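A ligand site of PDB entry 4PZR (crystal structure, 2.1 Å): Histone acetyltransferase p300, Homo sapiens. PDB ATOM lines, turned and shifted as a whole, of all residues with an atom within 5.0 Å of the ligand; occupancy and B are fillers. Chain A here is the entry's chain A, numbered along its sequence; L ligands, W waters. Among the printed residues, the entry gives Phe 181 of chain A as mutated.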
ATOM      1  N   SER A 110     -15.136  -8.667  18.899  1.00  0.00           N
ATOM      2  CA  SER A 110     -15.486  -7.792  20.026  1.00  0.00           C
ATOM      3  C   SER A 110     -14.253  -7.567  20.895  1.00  0.00           C
ATOM      4  O   SER A 110     -13.851  -6.437  21.157  1.00  0.00           O
ATOM      5  CB  SER A 110     -16.612  -8.396  20.875  1.00  0.00           C
ATOM      6  OG  SER A 110     -17.720  -8.820  20.090  1.00  0.00           O
ATOM      7  N   TYR A 111     -13.642  -8.675  21.336  1.00  0.00           N
ATOM      8  CA  TYR A 111     -12.424  -8.626  22.141  1.00  0.00           C
ATOM      9  C   TYR A 111     -11.791 -10.009  22.169  1.00  0.00           C
ATOM     10  O   TYR A 111     -12.455 -11.025  21.918  1.00  0.00           O
ATOM     11  CB  TYR A 111     -12.702  -8.131  23.574  1.00  0.00           C
ATOM     12  CG  TYR A 111     -14.123  -8.317  24.034  1.00  0.00           C
ATOM     13  CD1 TYR A 111     -14.963  -7.219  24.170  1.00  0.00           C
ATOM     14  CD2 TYR A 111     -14.636  -9.581  24.300  1.00  0.00           C
ATOM     15  CE1 TYR A 111     -16.284  -7.377  24.585  1.00  0.00           C
ATOM     16  CE2 TYR A 111     -15.959  -9.754  24.703  1.00  0.00           C
ATOM     17  CZ  TYR A 111     -16.777  -8.645  24.852  1.00  0.00           C
ATOM     18  OH  TYR A 111     -18.095  -8.797  25.258  1.00  0.00           O
ATOM     19  N   LEU A 112     -10.499 -10.039  22.436  1.00  0.00           N
ATOM     20  CA  LEU A 112      -9.768 -11.265  22.633  1.00  0.00           C
ATOM     21  C   LEU A 112      -8.860 -10.995  23.826  1.00  0.00           C
ATOM     22  O   LEU A 112      -8.614  -9.853  24.162  1.00  0.00           O
ATOM     23  CB  LEU A 112      -8.988 -11.674  21.368  1.00  0.00           C
ATOM     24  CG  LEU A 112      -7.850 -10.804  20.820  1.00  0.00           C
ATOM     25  CD1 LEU A 112      -6.537 -10.975  21.626  1.00  0.00           C
ATOM     26  CD2 LEU A 112      -7.613 -11.078  19.336  1.00  0.00           C
ATOM     27  N   ASP A 113      -8.397 -12.065  24.473  1.00  0.00           N
ATOM     28  CA  ASP A 113      -7.622 -11.921  25.697  1.00  0.00           C
ATOM     29  C   ASP A 113      -6.795 -13.195  25.819  1.00  0.00           C
ATOM     30  O   ASP A 113      -7.164 -14.213  25.245  1.00  0.00           O
ATOM     31  CB  ASP A 113      -8.558 -11.720  26.907  1.00  0.00           C
ATOM     32  CG  ASP A 113      -7.831 -11.271  28.175  1.00  0.00           C
ATOM     33  OD1 ASP A 113      -6.663 -10.842  28.093  1.00  0.00           O
ATOM     34  OD2 ASP A 113      -8.457 -11.323  29.259  1.00  0.00           O
ATOM     35  N   SER A 114      -5.704 -13.132  26.568  1.00  0.00           N
ATOM     36  CA  SER A 114      -4.882 -14.304  26.824  1.00  0.00           C
ATOM     37  C   SER A 114      -4.154 -14.205  28.155  1.00  0.00           C
ATOM     38  O   SER A 114      -4.018 -13.123  28.749  1.00  0.00           O
ATOM     39  CB  SER A 114      -3.844 -14.484  25.713  1.00  0.00           C
ATOM     40  OG  SER A 114      -2.928 -13.405  25.750  1.00  0.00           O
ATOM     41  N   LYS A 121       6.947 -21.247  25.377  1.00  0.00           N
ATOM     42  CA  LYS A 121       6.912 -19.800  25.186  1.00  0.00           C
ATOM     43  C   LYS A 121       7.132 -19.358  23.743  1.00  0.00           C
ATOM     44  O   LYS A 121       6.424 -18.473  23.236  1.00  0.00           O
ATOM     45  CB  LYS A 121       7.988 -19.128  26.052  1.00  0.00           C
ATOM     46  CG  LYS A 121       7.667 -19.095  27.523  1.00  0.00           C
ATOM     47  CD  LYS A 121       8.858 -18.525  28.328  1.00  0.00           C
ATOM     48  CE  LYS A 121       9.367 -17.215  27.747  1.00  0.00           C
ATOM     49  NZ  LYS A 121       9.974 -16.303  28.794  1.00  0.00           N
ATOM     50  N   ARG A 124       4.009 -19.378  21.521  1.00  0.00           N
ATOM     51  CA  ARG A 124       2.784 -18.726  21.994  1.00  0.00           C
ATOM     52  C   ARG A 124       2.158 -17.792  20.942  1.00  0.00           C
ATOM     53  O   ARG A 124       1.020 -17.977  20.556  1.00  0.00           O
ATOM     54  CB  ARG A 124       3.073 -17.938  23.284  1.00  0.00           C
ATOM     55  CG  ARG A 124       1.812 -17.350  23.952  1.00  0.00           C
ATOM     56  CD  ARG A 124       2.175 -16.398  25.123  1.00  0.00           C
ATOM     57  NE  ARG A 124       2.930 -15.259  24.611  1.00  0.00           N
ATOM     58  CZ  ARG A 124       4.260 -15.127  24.651  1.00  0.00           C
ATOM     59  NH1 ARG A 124       5.036 -16.066  25.198  1.00  0.00           N
ATOM     60  NH2 ARG A 124       4.816 -14.052  24.138  1.00  0.00           N
ATOM     61  N   THR A 125       2.919 -16.800  20.475  1.00  0.00           N
ATOM     62  CA  THR A 125       2.388 -15.826  19.533  1.00  0.00           C
ATOM     63  C   THR A 125       1.941 -16.500  18.229  1.00  0.00           C
ATOM     64  O   THR A 125       0.881 -16.192  17.686  1.00  0.00           O
ATOM     65  CB  THR A 125       3.411 -14.726  19.211  1.00  0.00           C
ATOM     66  OG1 THR A 125       3.678 -13.971  20.398  1.00  0.00           O
ATOM     67  CG2 THR A 125       2.882 -13.785  18.111  1.00  0.00           C
ATOM     68  N   TYR A 128      -1.517 -18.027  18.737  1.00  0.00           N
ATOM     69  CA  TYR A 128      -2.570 -17.011  18.695  1.00  0.00           C
ATOM     70  C   TYR A 128      -2.891 -16.650  17.241  1.00  0.00           C
ATOM     71  O   TYR A 128      -4.055 -16.591  16.836  1.00  0.00           O
ATOM     72  CB  TYR A 128      -2.152 -15.736  19.436  1.00  0.00           C
ATOM     73  CG  TYR A 128      -1.903 -15.854  20.922  1.00  0.00           C
ATOM     74  CD1 TYR A 128      -2.552 -16.824  21.689  1.00  0.00           C
ATOM     75  CD2 TYR A 128      -1.007 -14.990  21.574  1.00  0.00           C
ATOM     76  CE1 TYR A 128      -2.304 -16.929  23.072  1.00  0.00           C
ATOM     77  CE2 TYR A 128      -0.765 -15.082  22.940  1.00  0.00           C
ATOM     78  CZ  TYR A 128      -1.413 -16.049  23.685  1.00  0.00           C
ATOM     79  OH  TYR A 128      -1.170 -16.142  25.038  1.00  0.00           O
ATOM     80  N   TRP A 150     -10.832  -3.802  16.020  1.00  0.00           N
ATOM     81  CA  TRP A 150     -10.479  -2.596  16.736  1.00  0.00           C
ATOM     82  C   TRP A 150      -9.317  -2.902  17.675  1.00  0.00           C
ATOM     83  O   TRP A 150      -9.501  -3.510  18.722  1.00  0.00           O
ATOM     84  CB  TRP A 150     -11.698  -2.078  17.487  1.00  0.00           C
ATOM     85  CG  TRP A 150     -11.434  -0.939  18.398  1.00  0.00           C
ATOM     86  CD1 TRP A 150     -10.317  -0.156  18.444  1.00  0.00           C
ATOM     87  CD2 TRP A 150     -12.321  -0.435  19.409  1.00  0.00           C
ATOM     88  NE1 TRP A 150     -10.444   0.805  19.418  1.00  0.00           N
ATOM     89  CE2 TRP A 150     -11.671   0.655  20.020  1.00  0.00           C
ATOM     90  CE3 TRP A 150     -13.596  -0.799  19.837  1.00  0.00           C
ATOM     91  CZ2 TRP A 150     -12.265   1.383  21.066  1.00  0.00           C
ATOM     92  CZ3 TRP A 150     -14.190  -0.074  20.869  1.00  0.00           C
ATOM     93  CH2 TRP A 150     -13.521   1.004  21.474  1.00  0.00           C
ATOM     94  N   ALA A 151      -8.115  -2.484  17.294  1.00  0.00           N
ATOM     95  CA  ALA A 151      -6.901  -2.833  18.041  1.00  0.00           C
ATOM     96  C   ALA A 151      -6.791  -1.947  19.261  1.00  0.00           C
ATOM     97  O   ALA A 151      -6.190  -0.877  19.201  1.00  0.00           O
ATOM     98  CB  ALA A 151      -5.659  -2.689  17.139  1.00  0.00           C
ATOM     99  N   CYS A 152      -7.380  -2.380  20.358  1.00  0.00           N
ATOM    100  CA  CYS A 152      -7.366  -1.555  21.565  1.00  0.00           C
ATOM    101  C   CYS A 152      -6.966  -2.349  22.804  1.00  0.00           C
ATOM    102  O   CYS A 152      -7.748  -3.153  23.313  1.00  0.00           O
ATOM    103  CB  CYS A 152      -8.742  -0.907  21.791  1.00  0.00           C
ATOM    104  SG  CYS A 152      -8.749   0.241  23.196  1.00  0.00           S
ATOM    105  N   PRO A 153      -5.739  -2.108  23.298  1.00  0.00           N
ATOM    106  CA  PRO A 153      -5.307  -2.812  24.509  1.00  0.00           C
ATOM    107  C   PRO A 153      -6.085  -2.316  25.725  1.00  0.00           C
ATOM    108  O   PRO A 153      -6.558  -1.173  25.710  1.00  0.00           O
ATOM    109  CB  PRO A 153      -3.829  -2.463  24.611  1.00  0.00           C
ATOM    110  CG  PRO A 153      -3.670  -1.199  23.873  1.00  0.00           C
ATOM    111  CD  PRO A 153      -4.721  -1.167  22.801  1.00  0.00           C
ATOM    112  N   PRO A 154      -6.229  -3.163  26.761  1.00  0.00           N
ATOM    113  CA  PRO A 154      -6.978  -2.774  27.945  1.00  0.00           C
ATOM    114  C   PRO A 154      -6.235  -1.689  28.708  1.00  0.00           C
ATOM    115  O   PRO A 154      -5.017  -1.591  28.602  1.00  0.00           O
ATOM    116  CB  PRO A 154      -7.036  -4.073  28.755  1.00  0.00           C
ATOM    117  CG  PRO A 154      -5.801  -4.791  28.387  1.00  0.00           C
ATOM    118  CD  PRO A 154      -5.600  -4.489  26.916  1.00  0.00           C
ATOM    119  N   TYR A 160      -9.870  -7.960  29.978  1.00  0.00           N
ATOM    120  CA  TYR A 160     -10.938  -8.116  28.994  1.00  0.00           C
ATOM    121  C   TYR A 160     -11.782  -9.342  29.290  1.00  0.00           C
ATOM    122  O   TYR A 160     -13.012  -9.282  29.306  1.00  0.00           O
ATOM    123  CB  TYR A 160     -10.360  -8.178  27.582  1.00  0.00           C
ATOM    124  CG  TYR A 160     -10.017  -6.823  27.034  1.00  0.00           C
ATOM    125  CD1 TYR A 160     -10.498  -5.654  27.645  1.00  0.00           C
ATOM    126  CD2 TYR A 160      -9.236  -6.690  25.903  1.00  0.00           C
ATOM    127  CE1 TYR A 160     -10.181  -4.404  27.142  1.00  0.00           C
ATOM    128  CE2 TYR A 160      -8.921  -5.448  25.393  1.00  0.00           C
ATOM    129  CZ  TYR A 160      -9.398  -4.308  26.010  1.00  0.00           C
ATOM    130  OH  TYR A 160      -9.066  -3.086  25.489  1.00  0.00           O
ATOM    131  N   HIS A 165      -4.768 -10.976  35.523  1.00  0.00           N
ATOM    132  CA  HIS A 165      -3.658 -11.409  34.684  1.00  0.00           C
ATOM    133  C   HIS A 165      -2.407 -11.525  35.515  1.00  0.00           C
ATOM    134  O   HIS A 165      -2.310 -10.919  36.573  1.00  0.00           O
ATOM    135  CB  HIS A 165      -3.416 -10.425  33.541  1.00  0.00           C
ATOM    136  CG  HIS A 165      -4.298 -10.627  32.353  1.00  0.00           C
ATOM    137  ND1 HIS A 165      -5.665 -10.444  32.389  1.00  0.00           N
ATOM    138  CD2 HIS A 165      -4.004 -10.963  31.073  1.00  0.00           C
ATOM    139  CE1 HIS A 165      -6.173 -10.675  31.199  1.00  0.00           C
ATOM    140  NE2 HIS A 165      -5.180 -10.983  30.373  1.00  0.00           N
ATOM    141  N   GLN A 169       2.830 -10.096  33.081  1.00  0.00           N
ATOM    142  CA  GLN A 169       2.432 -10.159  31.672  1.00  0.00           C
ATOM    143  C   GLN A 169       2.276  -8.735  31.153  1.00  0.00           C
ATOM    144  O   GLN A 169       1.310  -8.063  31.484  1.00  0.00           O
ATOM    145  CB  GLN A 169       1.129 -10.945  31.473  1.00  0.00           C
ATOM    146  CG  GLN A 169       0.690 -11.032  29.988  1.00  0.00           C
ATOM    147  CD  GLN A 169      -0.556 -11.884  29.778  1.00  0.00           C
ATOM    148  OE1 GLN A 169      -0.756 -12.882  30.473  1.00  0.00           O
ATOM    149  NE2 GLN A 169      -1.404 -11.508  28.820  1.00  0.00           N
ATOM    150  N   LYS A 170       3.245  -8.267  30.373  1.00  0.00           N
ATOM    151  CA  LYS A 170       3.197  -6.911  29.866  1.00  0.00           C
ATOM    152  C   LYS A 170       2.005  -6.738  28.927  1.00  0.00           C
ATOM    153  O   LYS A 170       1.599  -7.668  28.245  1.00  0.00           O
ATOM    154  CB  LYS A 170       4.477  -6.553  29.125  1.00  0.00           C
ATOM    155  CG  LYS A 170       5.725  -6.532  30.027  1.00  0.00           C
ATOM    156  CD  LYS A 170       6.864  -5.780  29.348  1.00  0.00           C
ATOM    157  CE  LYS A 170       8.164  -5.865  30.161  1.00  0.00           C
ATOM    158  NZ  LYS A 170       8.698  -7.243  30.172  1.00  0.00           N
ATOM    159  N   ILE A 171       1.454  -5.530  28.929  1.00  0.00           N
ATOM    160  CA  ILE A 171       0.350  -5.177  28.047  1.00  0.00           C
ATOM    161  C   ILE A 171       0.891  -4.378  26.876  1.00  0.00           C
ATOM    162  O   ILE A 171       1.586  -3.377  27.072  1.00  0.00           O
ATOM    163  CB  ILE A 171      -0.714  -4.378  28.807  1.00  0.00           C
ATOM    164  CG1 ILE A 171      -1.242  -5.211  29.970  1.00  0.00           C
ATOM    165  CG2 ILE A 171      -1.837  -3.985  27.876  1.00  0.00           C
ATOM    166  CD1 ILE A 171      -2.402  -4.576  30.668  1.00  0.00           C
ATOM    167  N   PRO A 172       0.633  -4.835  25.641  1.00  0.00           N
ATOM    168  CA  PRO A 172       1.240  -4.092  24.530  1.00  0.00           C
ATOM    169  C   PRO A 172       0.648  -2.680  24.419  1.00  0.00           C
ATOM    170  O   PRO A 172      -0.512  -2.503  24.769  1.00  0.00           O
ATOM    171  CB  PRO A 172       0.876  -4.929  23.290  1.00  0.00           C
ATOM    172  CG  PRO A 172      -0.372  -5.642  23.688  1.00  0.00           C
ATOM    173  CD  PRO A 172      -0.233  -5.933  25.178  1.00  0.00           C
ATOM    174  N   LYS A 173       1.450  -1.722  23.987  1.00  0.00           N
ATOM    175  CA  LYS A 173       0.976  -0.398  23.628  1.00  0.00           C
ATOM    176  C   LYS A 173       0.317  -0.517  22.273  1.00  0.00           C
ATOM    177  O   LYS A 173       0.561  -1.487  21.553  1.00  0.00           O
ATOM    178  CB  LYS A 173       2.120   0.618  23.558  1.00  0.00           C
ATOM    179  CG  LYS A 173       2.957   0.778  24.831  1.00  0.00           C
ATOM    180  CD  LYS A 173       2.484   1.954  25.685  1.00  0.00           C
ATOM    181  CE  LYS A 173       3.428   2.154  26.860  1.00  0.00           C
ATOM    182  NZ  LYS A 173       2.929   3.151  27.843  1.00  0.00           N
ATOM    183  N   ARG A 176       2.433  -1.587  19.235  1.00  0.00           N
ATOM    184  CA  ARG A 176       2.861  -2.973  19.266  1.00  0.00           C
ATOM    185  C   ARG A 176       1.698  -3.906  18.907  1.00  0.00           C
ATOM    186  O   ARG A 176       1.875  -4.829  18.106  1.00  0.00           O
ATOM    187  CB  ARG A 176       3.439  -3.347  20.642  1.00  0.00           C
ATOM    188  CG  ARG A 176       3.811  -4.827  20.745  1.00  0.00           C
ATOM    189  CD  ARG A 176       4.316  -5.160  22.134  1.00  0.00           C
ATOM    190  NE  ARG A 176       5.600  -4.532  22.416  1.00  0.00           N
ATOM    191  CZ  ARG A 176       6.772  -5.036  22.012  1.00  0.00           C
ATOM    192  NH1 ARG A 176       6.807  -6.160  21.313  1.00  0.00           N
ATOM    193  NH2 ARG A 176       7.892  -4.404  22.312  1.00  0.00           N
ATOM    194  N   LEU A 177       0.506  -3.639  19.449  1.00  0.00           N
ATOM    195  CA  LEU A 177      -0.683  -4.446  19.148  1.00  0.00           C
ATOM    196  C   LEU A 177      -1.030  -4.349  17.664  1.00  0.00           C
ATOM    197  O   LEU A 177      -1.400  -5.343  17.007  1.00  0.00           O
ATOM    198  CB  LEU A 177      -1.876  -4.011  20.021  1.00  0.00           C
ATOM    199  CG  LEU A 177      -3.139  -4.841  19.836  1.00  0.00           C
ATOM    200  CD1 LEU A 177      -2.835  -6.312  20.080  1.00  0.00           C
ATOM    201  CD2 LEU A 177      -4.326  -4.373  20.733  1.00  0.00           C
ATOM    202  N   TRP A 180       1.332  -6.396  15.691  1.00  0.00           N
ATOM    203  CA  TRP A 180       0.927  -7.772  15.962  1.00  0.00           C
ATOM    204  C   TRP A 180      -0.194  -8.246  15.028  1.00  0.00           C
ATOM    205  O   TRP A 180      -0.049  -9.279  14.367  1.00  0.00           O
ATOM    206  CB  TRP A 180       0.476  -7.865  17.416  1.00  0.00           C
ATOM    207  CG  TRP A 180       0.258  -9.251  17.993  1.00  0.00           C
ATOM    208  CD1 TRP A 180       1.184 -10.055  18.593  1.00  0.00           C
ATOM    209  CD2 TRP A 180      -0.998  -9.937  18.086  1.00  0.00           C
ATOM    210  NE1 TRP A 180       0.593 -11.214  19.040  1.00  0.00           N
ATOM    211  CE2 TRP A 180      -0.756 -11.167  18.748  1.00  0.00           C
ATOM    212  CE3 TRP A 180      -2.303  -9.633  17.675  1.00  0.00           C
ATOM    213  CZ2 TRP A 180      -1.767 -12.098  18.993  1.00  0.00           C
ATOM    214  CZ3 TRP A 180      -3.313 -10.556  17.925  1.00  0.00           C
ATOM    215  CH2 TRP A 180      -3.038 -11.781  18.573  1.00  0.00           C
ATOM    216  N   PHE A 181      -1.280  -7.479  14.940  1.00  0.00           N
ATOM    217  CA  PHE A 181      -2.357  -7.801  14.011  1.00  0.00           C
ATOM    218  C   PHE A 181      -1.855  -7.801  12.552  1.00  0.00           C
ATOM    219  O   PHE A 181      -2.247  -8.658  11.751  1.00  0.00           O
ATOM    220  CB  PHE A 181      -3.556  -6.836  14.175  1.00  0.00           C
ATOM    221  CG  PHE A 181      -4.452  -7.159  15.334  1.00  0.00           C
ATOM    222  CD1 PHE A 181      -4.477  -6.344  16.463  1.00  0.00           C
ATOM    223  CD2 PHE A 181      -5.253  -8.312  15.318  1.00  0.00           C
ATOM    224  CE1 PHE A 181      -5.291  -6.641  17.534  1.00  0.00           C
ATOM    225  CE2 PHE A 181      -6.087  -8.610  16.396  1.00  0.00           C
ATOM    226  CZ  PHE A 181      -6.097  -7.779  17.515  1.00  0.00           C
HETATM  227  N1  LIG L   1       6.564  -3.080  26.592  1.00  0.00           N
HETATM  228  C1  LIG L   1       7.573  -3.874  26.296  1.00  0.00           C
HETATM  229  N2  LIG L   1       7.377  -5.126  25.893  1.00  0.00           N
HETATM  230  C2  LIG L   1       6.113  -5.619  25.797  1.00  0.00           C
HETATM  231  C3  LIG L   1       5.004  -4.816  26.090  1.00  0.00           C
HETATM  232  C4  LIG L   1       5.279  -3.478  26.509  1.00  0.00           C
HETATM  233  N3  LIG L   1       4.230  -2.582  26.831  1.00  0.00           N
HETATM  234  N4  LIG L   1       3.908  -5.594  25.878  1.00  0.00           N
HETATM  235  C5  LIG L   1       4.324  -6.818  25.475  1.00  0.00           C
HETATM  236  N5  LIG L   1       5.646  -6.840  25.419  1.00  0.00           N
HETATM  237  C6  LIG L   1       6.488  -7.893  25.054  1.00  0.00           C
HETATM  238  C7  LIG L   1       6.052  -9.164  25.766  1.00  0.00           C
HETATM  239  O1  LIG L   1       6.659  -9.209  27.032  1.00  0.00           O
HETATM  240  C8  LIG L   1       6.502 -10.229  24.836  1.00  0.00           C
HETATM  241  O2  LIG L   1       7.892 -10.504  25.137  1.00  0.00           O
HETATM  242  P1  LIG L   1       8.524 -11.893  24.801  1.00  0.00           P
HETATM  243  O3  LIG L   1       8.057 -12.841  25.883  1.00  0.00           O
HETATM  244  O4  LIG L   1      10.036 -11.774  24.848  1.00  0.00           O
HETATM  245  O5  LIG L   1       8.085 -12.411  23.422  1.00  0.00           O
HETATM  246  C9  LIG L   1       6.420  -9.638  23.522  1.00  0.00           C
HETATM  247  O6  LIG L   1       6.369  -8.180  23.658  1.00  0.00           O
HETATM  248  C10 LIG L   1       5.159 -10.093  22.782  1.00  0.00           C
HETATM  249  O7  LIG L   1       4.041  -9.873  23.656  1.00  0.00           O
HETATM  250  P2  LIG L   1       2.634  -9.439  23.028  1.00  0.00           P
HETATM  251  O8  LIG L   1       2.765  -8.254  22.116  1.00  0.00           O
HETATM  252  O9  LIG L   1       1.675  -9.180  24.149  1.00  0.00           O
HETATM  253  O10 LIG L   1       2.181 -10.651  22.075  1.00  0.00           O
HETATM  254  P3  LIG L   1       1.466 -11.995  22.515  1.00  0.00           P
HETATM  255  O11 LIG L   1       1.283 -12.852  21.274  1.00  0.00           O
HETATM  256  O12 LIG L   1       2.263 -12.712  23.570  1.00  0.00           O
HETATM  257  O13 LIG L   1       0.025 -11.646  23.075  1.00  0.00           O
HETATM  258  C11 LIG L   1      -2.168 -10.547  22.997  1.00  0.00           C
HETATM  259  C12 LIG L   1      -0.779 -10.753  22.291  1.00  0.00           C
HETATM  260  C13 LIG L   1      -2.897  -9.335  22.343  1.00  0.00           C
HETATM  261  C14 LIG L   1      -3.041 -11.866  22.899  1.00  0.00           C
HETATM  262  C15 LIG L   1      -1.820 -10.223  24.506  1.00  0.00           C
HETATM  263  O14 LIG L   1      -0.952  -9.166  24.568  1.00  0.00           O
HETATM  264  C16 LIG L   1      -3.077  -9.990  25.347  1.00  0.00           C
HETATM  265  O15 LIG L   1      -3.781 -10.938  25.708  1.00  0.00           O
HETATM  266  N6  LIG L   1      -3.429  -8.627  25.700  1.00  0.00           N
HETATM  267  C17 LIG L   1      -4.556  -8.327  26.503  1.00  0.00           C
HETATM  268  C18 LIG L   1      -5.826  -8.240  25.698  1.00  0.00           C
HETATM  269  C19 LIG L   1      -5.732  -7.410  24.390  1.00  0.00           C
HETATM  270  O16 LIG L   1      -4.937  -6.494  24.287  1.00  0.00           O
HETATM  271  N7  LIG L   1      -6.556  -7.714  23.241  1.00  0.00           N
HETATM  272  C20 LIG L   1      -6.408  -6.942  22.016  1.00  0.00           C
HETATM  273  C21 LIG L   1      -7.591  -5.954  21.791  1.00  0.00           C
HETATM  274  S1  LIG L   1      -9.011  -6.853  21.213  1.00  0.00           S
HETATM  275  O   HOH W   1      10.132 -13.782  27.588  1.00  0.00           O
HETATM  276  O   HOH W   2       7.942 -15.612  24.946  1.00  0.00           O
HETATM  277  O   HOH W   3       2.756  -9.540  26.686  1.00  0.00           O
HETATM  278  O   HOH W   4      -0.658  -8.855  27.360  1.00  0.00           O
HETATM  279  O   HOH W   5      11.204 -14.069  23.973  1.00  0.00           O
HETATM  280  O   HOH W   6       4.411  -7.986  19.984  1.00  0.00           O
HETATM  281  O   HOH W   7       6.420  -0.782  24.929  1.00  0.00           O
HETATM  282  O   HOH W   8       9.459  -9.028  27.595  1.00  0.00           O
HETATM  283  O   HOH W   9       9.875  -6.312  25.675  1.00  0.00           O
HETATM  284  O   HOH W  10       1.849 -12.192  26.272  1.00  0.00           O
HETATM  285  O   HOH W  11       0.504  -7.351  20.829  1.00  0.00           O
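Water W6 lies within hydrogen-bond range of an oxygen (O8) of the ligand and the guanidinium group (NH1) of Arg 176. Water W3 bridges the backbone carbonyl oxygen of Lys 170 (2.7 Å) and an oxygen (O9) of the ligand (2.8 Å). Water W4 lies within hydrogen-bond range of the backbone carbonyl oxygen of Lys 170, an oxygen (O14) of the ligand and the side-chain amide nitrogen of Gln 169. Water W1 bridges NZ of Lys 121 (2.8 Å) and O3 of the ligand (2.8 Å). Water W8 lies within hydrogen-bond range of O1 of the ligand (2.9 Å) and NZ of Lys 170 (3.2 Å). Water W2 bridges O3 of the ligand (2.9 Å) and NH1 of Arg 124 (3.0 Å).
The backbone nitrogen of Pro 172 lies close to a nitrogen (N4) of the ligand, at 3.4 Å. Tyr 111 touches the ligand. OD1 of Asp 113 touches C18 of the ligand (3.6 Å). CD2 of Tyr 128 touches O11 of the ligand, 3.1 Å away. Cys 152 touches the ligand (O to C21, 3.2 Å). CA of Pro 153 touches O16 of the ligand, at 3.7 Å. Pro 154 touches the ligand. CD2 of Tyr 160 touches C18 of the ligand, at 3.8 Å. NE2 of Gln 169 touches O15 of the ligand, at 3.96 Å. Lys 170 touches the ligand (CB to N4, 3.4 Å). CD2 of Leu 177 touches C20 of the ligand, at 3.5 Å. Within 4 Å of the ligand: Tyr 111, Leu 112, Asp 113, Ser 114, Arg 124, Thr 125, Tyr 128, Cys 152, Pro 153, Pro 154, Tyr 160, Gln 169, Lys 170, Ile 171, Pro 172, Arg 176, Leu 177 and Trp 180. The nearest printed residue that does not touch the ligand is Lys 173 (4.1 Å).
The indole nitrogen (NE1) of Trp 180 is in hydrogen-bond range of an oxygen (O11) of the ligand. An oxygen (O6) of the ligand lies within hydrogen-bond range of the guanidinium group of Arg 176, at 3.1 Å. O of Ile 171 is in hydrogen-bond range of N3 of the ligand (2.8 Å). N of Leu 112 lies close to S1 of the ligand (3.7 Å). The guanidinium group (NE) of Arg 124 is in salt-bridge range of an oxygen (O12) of the ligand (2.8 Å). The backbone carbonyl oxygen (O) of Leu 112 sits at hydrogen-bond distance from a nitrogen (N7) of the ligand, at 3.1 Å. An oxygen (O15) of the ligand lies within hydrogen-bond range of the side-chain hydroxyl (OG) of Ser 114, at 2.6 Å. The side-chain hydroxyl of Thr 125 is in hydrogen-bond range of an oxygen (O11) of the ligand, 2.8 Å away. An oxygen (O15) of the ligand lies within hydrogen-bond range of the backbone NH (N) of Ser 114.
O of Pro 153 sits close to OH of Tyr 160 (3.2 Å). The side-chain hydroxyl (OG) of Ser 114 sits close to the side-chain hydroxyl (OH) of Tyr 128 (3.3 Å). The backbone carbonyl oxygen of Cys 152 sits at hydrogen-bond distance from the side-chain hydroxyl of Tyr 160 (2.5 Å). The backbone carbonyl oxygen (O) of Lys 121 sits close to the guanidinium group (NH1) of Arg 124 (3.4 Å). NE2 of His 165 is in hydrogen-bond range of OD1 of Asp 113, 2.7 Å away. The backbone carbonyl oxygen of Ser 114 lies within hydrogen-bond range of the side-chain amide nitrogen of Gln 169 (3.1 Å). The backbone carbonyl oxygen (O) of Ser 114 sits at hydrogen-bond distance from a ring nitrogen (NE2) of His 165 (2.9 Å).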
